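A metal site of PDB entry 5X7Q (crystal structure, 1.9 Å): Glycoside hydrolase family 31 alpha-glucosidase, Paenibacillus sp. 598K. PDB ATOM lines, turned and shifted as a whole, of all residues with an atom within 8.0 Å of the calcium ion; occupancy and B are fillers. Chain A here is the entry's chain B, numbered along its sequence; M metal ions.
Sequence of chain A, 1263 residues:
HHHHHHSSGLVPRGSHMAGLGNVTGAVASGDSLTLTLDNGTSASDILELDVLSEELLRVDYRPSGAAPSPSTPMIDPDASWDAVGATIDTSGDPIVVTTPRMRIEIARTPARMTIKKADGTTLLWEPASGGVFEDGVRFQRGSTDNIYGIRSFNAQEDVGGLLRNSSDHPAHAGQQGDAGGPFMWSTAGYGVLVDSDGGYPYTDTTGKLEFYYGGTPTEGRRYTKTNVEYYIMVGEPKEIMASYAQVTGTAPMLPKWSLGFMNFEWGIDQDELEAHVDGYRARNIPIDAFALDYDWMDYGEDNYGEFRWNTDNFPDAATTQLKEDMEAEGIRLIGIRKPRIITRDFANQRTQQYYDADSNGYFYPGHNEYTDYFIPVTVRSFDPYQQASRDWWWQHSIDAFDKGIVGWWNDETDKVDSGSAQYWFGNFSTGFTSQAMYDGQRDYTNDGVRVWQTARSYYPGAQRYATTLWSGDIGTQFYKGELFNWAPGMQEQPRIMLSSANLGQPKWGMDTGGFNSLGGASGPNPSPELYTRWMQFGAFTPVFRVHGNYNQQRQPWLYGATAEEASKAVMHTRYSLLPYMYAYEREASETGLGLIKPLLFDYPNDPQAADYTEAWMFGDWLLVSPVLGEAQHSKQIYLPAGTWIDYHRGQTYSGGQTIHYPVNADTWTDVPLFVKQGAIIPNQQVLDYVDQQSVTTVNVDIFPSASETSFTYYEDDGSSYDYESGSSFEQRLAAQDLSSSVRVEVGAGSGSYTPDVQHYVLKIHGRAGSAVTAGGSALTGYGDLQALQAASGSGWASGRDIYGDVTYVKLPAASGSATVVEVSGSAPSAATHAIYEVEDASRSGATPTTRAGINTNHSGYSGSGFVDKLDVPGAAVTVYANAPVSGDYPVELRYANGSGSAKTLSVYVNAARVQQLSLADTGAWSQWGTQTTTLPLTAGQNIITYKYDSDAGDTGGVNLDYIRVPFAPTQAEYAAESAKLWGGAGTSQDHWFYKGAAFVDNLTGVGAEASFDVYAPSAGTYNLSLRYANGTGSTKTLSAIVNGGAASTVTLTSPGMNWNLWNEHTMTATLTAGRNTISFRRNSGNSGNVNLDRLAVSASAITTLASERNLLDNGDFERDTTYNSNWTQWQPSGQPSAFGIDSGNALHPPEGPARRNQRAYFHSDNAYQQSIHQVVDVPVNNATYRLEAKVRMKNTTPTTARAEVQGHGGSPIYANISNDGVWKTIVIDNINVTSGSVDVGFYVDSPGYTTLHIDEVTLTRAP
OD2 of Asp 1255 sits close to N of Ala 1154 (2.9 Å). The side-chain amide nitrogen (NE2) of Gln 1158 sits at hydrogen-bond distance from the backbone carbonyl oxygen (O) of Phe 1117. The backbone carbonyl oxygen (O) of Arg 1119 sits at hydrogen-bond distance from the side-chain amide nitrogen (NE2) of Gln 1158, at 3.0 Å. N of Asn 1157 sits at hydrogen-bond distance from OE1 of Glu 1118 (3.0 Å). The side-chain carboxylate (OE1) of Glu 1118 is in salt-bridge range of the guanidinium group (NH1) of Arg 1156, 2.7 Å away. N of Glu 1118 lies within hydrogen-bond range of OD1 of Asn 1114, 3.0 Å away. The guanidinium group of Arg 1155 is in salt-bridge range of the side-chain carboxylate of Asp 666, at 2.9 Å.
The nearest printed residue that does not touch the calcium ion is Pro 1153 (4.4 Å).
The calcium ion is bound by the side-chain carboxylate (OD1) of Asp 1255 (2.3 Å), the backbone carbonyl oxygen (O) of Gln 1158 (2.3 Å), the side-chain carboxylate (OE2) of Glu 1118 (2.4 Å), the backbone carbonyl oxygen (O) of Asp 1116 (2.5 Å), the side-chain carboxylate (OD2) of Asp 1255 (2.7 Å), the side-chain carboxylate (OE2) of Glu 1256 (2.7 Å) and the backbone carbonyl oxygen (O) of Arg 1155 (2.8 Å). The calcium ion has seven donor atoms within binding distance.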
ATOM      1  N   THR A 562     -32.850  23.695  30.879  1.00  0.00           N
ATOM      2  CA  THR A 562     -31.991  23.979  32.032  1.00  0.00           C
ATOM      3  C   THR A 562     -32.588  25.140  32.833  1.00  0.00           C
ATOM      4  O   THR A 562     -32.757  25.040  34.057  1.00  0.00           O
ATOM      5  CB  THR A 562     -30.560  24.294  31.645  1.00  0.00           C
ATOM      6  OG1 THR A 562     -30.026  23.203  30.880  1.00  0.00           O
ATOM      7  CG2 THR A 562     -29.692  24.485  32.885  1.00  0.00           C
ATOM      8  N   ASP A 666     -21.686  23.330  32.941  1.00  0.00           N
ATOM      9  CA  ASP A 666     -22.506  22.613  31.983  1.00  0.00           C
ATOM     10  C   ASP A 666     -23.958  22.471  32.449  1.00  0.00           C
ATOM     11  O   ASP A 666     -24.882  22.596  31.660  1.00  0.00           O
ATOM     12  CB  ASP A 666     -21.903  21.242  31.700  1.00  0.00           C
ATOM     13  CG  ASP A 666     -22.650  20.490  30.610  1.00  0.00           C
ATOM     14  OD1 ASP A 666     -22.968  21.095  29.559  1.00  0.00           O
ATOM     15  OD2 ASP A 666     -22.981  19.318  30.832  1.00  0.00           O
ATOM     16  N   ASN A1114     -19.036  18.806  20.653  1.00  0.00           N
ATOM     17  CA  ASN A1114     -19.985  19.936  20.631  1.00  0.00           C
ATOM     18  C   ASN A1114     -21.382  19.535  20.142  1.00  0.00           C
ATOM     19  O   ASN A1114     -22.038  20.271  19.383  1.00  0.00           O
ATOM     20  CB  ASN A1114     -19.434  21.083  19.755  1.00  0.00           C
ATOM     21  CG  ASN A1114     -20.156  22.407  19.990  1.00  0.00           C
ATOM     22  OD1 ASN A1114     -20.561  22.716  21.103  1.00  0.00           O
ATOM     23  ND2 ASN A1114     -20.295  23.222  18.936  1.00  0.00           N
ATOM     24  N   GLY A1115     -21.858  18.383  20.600  1.00  0.00           N
ATOM     25  CA  GLY A1115     -23.163  17.865  20.170  1.00  0.00           C
ATOM     26  C   GLY A1115     -24.341  18.673  20.693  1.00  0.00           C
ATOM     27  O   GLY A1115     -25.440  18.604  20.145  1.00  0.00           O
ATOM     28  N   ASP A1116     -24.092  19.426  21.769  1.00  0.00           N
ATOM     29  CA  ASP A1116     -25.077  20.322  22.357  1.00  0.00           C
ATOM     30  C   ASP A1116     -24.971  21.764  21.856  1.00  0.00           C
ATOM     31  O   ASP A1116     -25.747  22.625  22.303  1.00  0.00           O
ATOM     32  CB  ASP A1116     -25.010  20.275  23.895  1.00  0.00           C
ATOM     33  CG  ASP A1116     -23.606  20.549  24.448  1.00  0.00           C
ATOM     34  OD1 ASP A1116     -22.721  21.028  23.710  1.00  0.00           O
ATOM     35  OD2 ASP A1116     -23.395  20.272  25.658  1.00  0.00           O
ATOM     36  N   PHE A1117     -24.020  22.027  20.950  1.00  0.00           N
ATOM     37  CA  PHE A1117     -23.755  23.346  20.392  1.00  0.00           C
ATOM     38  C   PHE A1117     -23.478  24.420  21.448  1.00  0.00           C
ATOM     39  O   PHE A1117     -23.760  25.599  21.240  1.00  0.00           O
ATOM     40  CB  PHE A1117     -24.913  23.768  19.477  1.00  0.00           C
ATOM     41  CG  PHE A1117     -25.243  22.740  18.429  1.00  0.00           C
ATOM     42  CD1 PHE A1117     -24.445  22.625  17.296  1.00  0.00           C
ATOM     43  CD2 PHE A1117     -26.317  21.893  18.593  1.00  0.00           C
ATOM     44  CE1 PHE A1117     -24.736  21.666  16.340  1.00  0.00           C
ATOM     45  CE2 PHE A1117     -26.636  20.959  17.633  1.00  0.00           C
ATOM     46  CZ  PHE A1117     -25.820  20.829  16.506  1.00  0.00           C
ATOM     47  N   GLU A1118     -22.901  24.000  22.578  1.00  0.00           N
ATOM     48  CA  GLU A1118     -22.681  24.914  23.715  1.00  0.00           C
ATOM     49  C   GLU A1118     -21.368  25.659  23.650  1.00  0.00           C
ATOM     50  O   GLU A1118     -21.161  26.602  24.416  1.00  0.00           O
ATOM     51  CB  GLU A1118     -22.778  24.155  25.036  1.00  0.00           C
ATOM     52  CG  GLU A1118     -24.197  23.703  25.326  1.00  0.00           C
ATOM     53  CD  GLU A1118     -25.170  24.863  25.400  1.00  0.00           C
ATOM     54  OE1 GLU A1118     -24.856  25.908  26.034  1.00  0.00           O
ATOM     55  OE2 GLU A1118     -26.267  24.729  24.813  1.00  0.00           O
ATOM     56  N   ARG A1119     -20.482  25.270  22.750  1.00  0.00           N
ATOM     57  CA  ARG A1119     -19.209  25.956  22.660  1.00  0.00           C
ATOM     58  C   ARG A1119     -19.419  27.420  22.244  1.00  0.00           C
ATOM     59  O   ARG A1119     -20.269  27.712  21.401  1.00  0.00           O
ATOM     60  CB  ARG A1119     -18.294  25.235  21.681  1.00  0.00           C
ATOM     61  CG  ARG A1119     -16.865  25.756  21.611  1.00  0.00           C
ATOM     62  CD  ARG A1119     -15.981  24.748  20.881  1.00  0.00           C
ATOM     63  NE  ARG A1119     -16.092  23.450  21.555  1.00  0.00           N
ATOM     64  CZ  ARG A1119     -15.903  22.254  21.003  1.00  0.00           C
ATOM     65  NH1 ARG A1119     -15.536  22.128  19.726  1.00  0.00           N
ATOM     66  NH2 ARG A1119     -16.099  21.173  21.742  1.00  0.00           N
ATOM     67  N   ILE A1141     -25.489  29.140  15.085  1.00  0.00           N
ATOM     68  CA  ILE A1141     -25.726  28.700  16.450  1.00  0.00           C
ATOM     69  C   ILE A1141     -25.860  29.966  17.292  1.00  0.00           C
ATOM     70  O   ILE A1141     -24.987  30.824  17.242  1.00  0.00           O
ATOM     71  CB  ILE A1141     -24.562  27.865  17.004  1.00  0.00           C
ATOM     72  CG1 ILE A1141     -24.356  26.557  16.199  1.00  0.00           C
ATOM     73  CG2 ILE A1141     -24.774  27.534  18.480  1.00  0.00           C
ATOM     74  CD1 ILE A1141     -22.932  26.036  16.267  1.00  0.00           C
ATOM     75  N   ASP A1142     -26.972  30.069  18.029  1.00  0.00           N
ATOM     76  CA  ASP A1142     -27.123  31.099  19.077  1.00  0.00           C
ATOM     77  C   ASP A1142     -28.211  30.649  20.078  1.00  0.00           C
ATOM     78  O   ASP A1142     -28.601  29.487  20.057  1.00  0.00           O
ATOM     79  CB  ASP A1142     -27.396  32.481  18.465  1.00  0.00           C
ATOM     80  CG  ASP A1142     -28.633  32.537  17.601  1.00  0.00           C
ATOM     81  OD1 ASP A1142     -29.717  32.060  18.021  1.00  0.00           O
ATOM     82  OD2 ASP A1142     -28.517  33.093  16.486  1.00  0.00           O
ATOM     83  N   GLY A1152     -35.969  29.213  22.325  1.00  0.00           N
ATOM     84  CA  GLY A1152     -34.780  28.910  23.116  1.00  0.00           C
ATOM     85  C   GLY A1152     -34.130  27.583  22.755  1.00  0.00           C
ATOM     86  O   GLY A1152     -34.567  26.894  21.821  1.00  0.00           O
ATOM     87  N   PRO A1153     -33.076  27.202  23.491  1.00  0.00           N
ATOM     88  CA  PRO A1153     -32.431  25.898  23.317  1.00  0.00           C
ATOM     89  C   PRO A1153     -33.245  24.790  23.960  1.00  0.00           C
ATOM     90  O   PRO A1153     -34.179  25.064  24.729  1.00  0.00           O
ATOM     91  CB  PRO A1153     -31.077  26.079  24.012  1.00  0.00           C
ATOM     92  CG  PRO A1153     -31.355  27.091  25.071  1.00  0.00           C
ATOM     93  CD  PRO A1153     -32.475  27.964  24.593  1.00  0.00           C
ATOM     94  N   ALA A1154     -32.922  23.538  23.634  1.00  0.00           N
ATOM     95  CA  ALA A1154     -33.496  22.405  24.345  1.00  0.00           C
ATOM     96  C   ALA A1154     -32.876  22.299  25.752  1.00  0.00           C
ATOM     97  O   ALA A1154     -33.560  21.973  26.704  1.00  0.00           O
ATOM     98  CB  ALA A1154     -33.283  21.115  23.571  1.00  0.00           C
ATOM     99  N   ARG A1155     -31.566  22.516  25.835  1.00  0.00           N
ATOM    100  CA  ARG A1155     -30.824  22.441  27.099  1.00  0.00           C
ATOM    101  C   ARG A1155     -29.719  23.482  27.075  1.00  0.00           C
ATOM    102  O   ARG A1155     -29.130  23.794  26.035  1.00  0.00           O
ATOM    103  CB  ARG A1155     -30.241  21.046  27.352  1.00  0.00           C
ATOM    104  CG  ARG A1155     -29.745  20.792  28.787  1.00  0.00           C
ATOM    105  CD  ARG A1155     -28.919  19.515  28.908  1.00  0.00           C
ATOM    106  NE  ARG A1155     -27.607  19.746  28.286  1.00  0.00           N
ATOM    107  CZ  ARG A1155     -26.577  20.390  28.844  1.00  0.00           C
ATOM    108  NH1 ARG A1155     -26.661  20.888  30.082  1.00  0.00           N
ATOM    109  NH2 ARG A1155     -25.458  20.558  28.136  1.00  0.00           N
ATOM    110  N   ARG A1156     -29.426  24.003  28.261  1.00  0.00           N
ATOM    111  CA  ARG A1156     -28.382  24.978  28.460  1.00  0.00           C
ATOM    112  C   ARG A1156     -28.623  26.277  27.645  1.00  0.00           C
ATOM    113  O   ARG A1156     -29.708  26.831  27.725  1.00  0.00           O
ATOM    114  CB  ARG A1156     -27.012  24.328  28.325  1.00  0.00           C
ATOM    115  CG  ARG A1156     -25.953  25.062  29.114  1.00  0.00           C
ATOM    116  CD  ARG A1156     -24.587  24.437  29.054  1.00  0.00           C
ATOM    117  NE  ARG A1156     -23.611  25.271  29.768  1.00  0.00           N
ATOM    118  CZ  ARG A1156     -23.004  26.332  29.261  1.00  0.00           C
ATOM    119  NH1 ARG A1156     -23.218  26.718  27.996  1.00  0.00           N
ATOM    120  NH2 ARG A1156     -22.164  27.044  30.014  1.00  0.00           N
ATOM    121  N   ASN A1157     -27.640  26.763  26.887  1.00  0.00           N
ATOM    122  CA  ASN A1157     -27.643  28.137  26.382  1.00  0.00           C
ATOM    123  C   ASN A1157     -27.853  28.288  24.879  1.00  0.00           C
ATOM    124  O   ASN A1157     -28.363  29.322  24.444  1.00  0.00           O
ATOM    125  CB  ASN A1157     -26.313  28.833  26.738  1.00  0.00           C
ATOM    126  CG  ASN A1157     -26.482  30.326  26.973  1.00  0.00           C
ATOM    127  OD1 ASN A1157     -27.525  30.795  27.436  1.00  0.00           O
ATOM    128  ND2 ASN A1157     -25.433  31.081  26.666  1.00  0.00           N
ATOM    129  N   GLN A1158     -27.506  27.276  24.099  1.00  0.00           N
ATOM    130  CA  GLN A1158     -27.397  27.429  22.649  1.00  0.00           C
ATOM    131  C   GLN A1158     -28.023  26.249  21.902  1.00  0.00           C
ATOM    132  O   GLN A1158     -28.172  25.142  22.424  1.00  0.00           O
ATOM    133  CB  GLN A1158     -25.936  27.630  22.249  1.00  0.00           C
ATOM    134  CG  GLN A1158     -25.441  29.053  22.477  1.00  0.00           C
ATOM    135  CD  GLN A1158     -23.959  29.280  22.230  1.00  0.00           C
ATOM    136  OE1 GLN A1158     -23.519  30.419  22.317  1.00  0.00           O
ATOM    137  NE2 GLN A1158     -23.189  28.222  21.923  1.00  0.00           N
ATOM    138  N   ARG A1159     -28.390  26.514  20.643  1.00  0.00           N
ATOM    139  CA  ARG A1159     -28.849  25.463  19.759  1.00  0.00           C
ATOM    140  C   ARG A1159     -28.569  25.872  18.330  1.00  0.00           C
ATOM    141  O   ARG A1159     -28.526  27.073  18.006  1.00  0.00           O
ATOM    142  CB  ARG A1159     -30.337  25.176  19.957  1.00  0.00           C
ATOM    143  CG  ARG A1159     -31.325  26.192  19.390  1.00  0.00           C
ATOM    144  CD  ARG A1159     -31.355  27.512  20.165  1.00  0.00           C
ATOM    145  NE  ARG A1159     -32.366  28.428  19.641  1.00  0.00           N
ATOM    146  CZ  ARG A1159     -32.238  29.172  18.550  1.00  0.00           C
ATOM    147  NH1 ARG A1159     -31.114  29.140  17.809  1.00  0.00           N
ATOM    148  NH2 ARG A1159     -33.233  29.959  18.171  1.00  0.00           N
ATOM    149  N   ALA A1160     -28.351  24.878  17.477  1.00  0.00           N
ATOM    150  CA  ALA A1160     -28.168  25.133  16.047  1.00  0.00           C
ATOM    151  C   ALA A1160     -29.498  25.518  15.453  1.00  0.00           C
ATOM    152  O   ALA A1160     -30.557  25.094  15.941  1.00  0.00           O
ATOM    153  CB  ALA A1160     -27.594  23.904  15.352  1.00  0.00           C
ATOM    154  N   TRP A1223     -40.253  21.149  20.623  1.00  0.00           N
ATOM    155  CA  TRP A1223     -39.067  20.297  20.765  1.00  0.00           C
ATOM    156  C   TRP A1223     -39.520  18.835  20.826  1.00  0.00           C
ATOM    157  O   TRP A1223     -40.423  18.503  21.568  1.00  0.00           O
ATOM    158  CB  TRP A1223     -38.276  20.623  22.040  1.00  0.00           C
ATOM    159  CG  TRP A1223     -37.393  21.804  21.937  1.00  0.00           C
ATOM    160  CD1 TRP A1223     -37.521  22.992  22.620  1.00  0.00           C
ATOM    161  CD2 TRP A1223     -36.219  21.933  21.122  1.00  0.00           C
ATOM    162  NE1 TRP A1223     -36.483  23.836  22.268  1.00  0.00           N
ATOM    163  CE2 TRP A1223     -35.693  23.212  21.344  1.00  0.00           C
ATOM    164  CE3 TRP A1223     -35.566  21.078  20.206  1.00  0.00           C
ATOM    165  CZ2 TRP A1223     -34.533  23.660  20.709  1.00  0.00           C
ATOM    166  CZ3 TRP A1223     -34.417  21.520  19.589  1.00  0.00           C
ATOM    167  CH2 TRP A1223     -33.911  22.804  19.833  1.00  0.00           C
ATOM    168  N   ILE A1254     -31.862  22.392  16.245  1.00  0.00           N
ATOM    169  CA  ILE A1254     -31.243  21.136  16.569  1.00  0.00           C
ATOM    170  C   ILE A1254     -30.445  21.340  17.850  1.00  0.00           C
ATOM    171  O   ILE A1254     -29.693  22.313  17.981  1.00  0.00           O
ATOM    172  CB  ILE A1254     -30.287  20.652  15.463  1.00  0.00           C
ATOM    173  CG1 ILE A1254     -30.960  20.685  14.078  1.00  0.00           C
ATOM    174  CG2 ILE A1254     -29.776  19.261  15.786  1.00  0.00           C
ATOM    175  CD1 ILE A1254     -29.962  20.810  12.941  1.00  0.00           C
ATOM    176  N   ASP A1255     -30.609  20.412  18.781  1.00  0.00           N
ATOM    177  CA  ASP A1255     -29.856  20.475  20.038  1.00  0.00           C
ATOM    178  C   ASP A1255     -29.604  19.092  20.659  1.00  0.00           C
ATOM    179  O   ASP A1255     -30.221  18.102  20.282  1.00  0.00           O
ATOM    180  CB  ASP A1255     -30.606  21.396  21.001  1.00  0.00           C
ATOM    181  CG  ASP A1255     -29.717  22.016  22.047  1.00  0.00           C
ATOM    182  OD1 ASP A1255     -28.480  21.782  22.011  1.00  0.00           O
ATOM    183  OD2 ASP A1255     -30.232  22.723  22.935  1.00  0.00           O
ATOM    184  N   GLU A1256     -28.687  19.045  21.606  1.00  0.00           N
ATOM    185  CA  GLU A1256     -28.476  17.873  22.461  1.00  0.00           C
ATOM    186  C   GLU A1256     -28.298  16.583  21.639  1.00  0.00           C
ATOM    187  O   GLU A1256     -28.910  15.552  21.910  1.00  0.00           O
ATOM    188  CB  GLU A1256     -29.616  17.760  23.474  1.00  0.00           C
ATOM    189  CG  GLU A1256     -29.802  18.994  24.371  1.00  0.00           C
ATOM    190  CD  GLU A1256     -28.491  19.553  24.924  1.00  0.00           C
ATOM    191  OE1 GLU A1256     -27.822  18.863  25.699  1.00  0.00           O
ATOM    192  OE2 GLU A1256     -28.108  20.707  24.615  1.00  0.00           O
ATOM    193  N   VAL A1257     -27.426  16.663  20.645  1.00  0.00           N
ATOM    194  CA  VAL A1257     -27.142  15.523  19.762  1.00  0.00           C
ATOM    195  C   VAL A1257     -26.148  14.618  20.479  1.00  0.00           C
ATOM    196  O   VAL A1257     -25.105  15.094  20.947  1.00  0.00           O
ATOM    197  CB  VAL A1257     -26.541  15.969  18.409  1.00  0.00           C
ATOM    198  CG1 VAL A1257     -26.501  14.791  17.428  1.00  0.00           C
ATOM    199  CG2 VAL A1257     -27.347  17.094  17.794  1.00  0.00           C
HETATM  200 CA    CA M   1     -27.695  23.219  23.681  1.00  0.00          CA
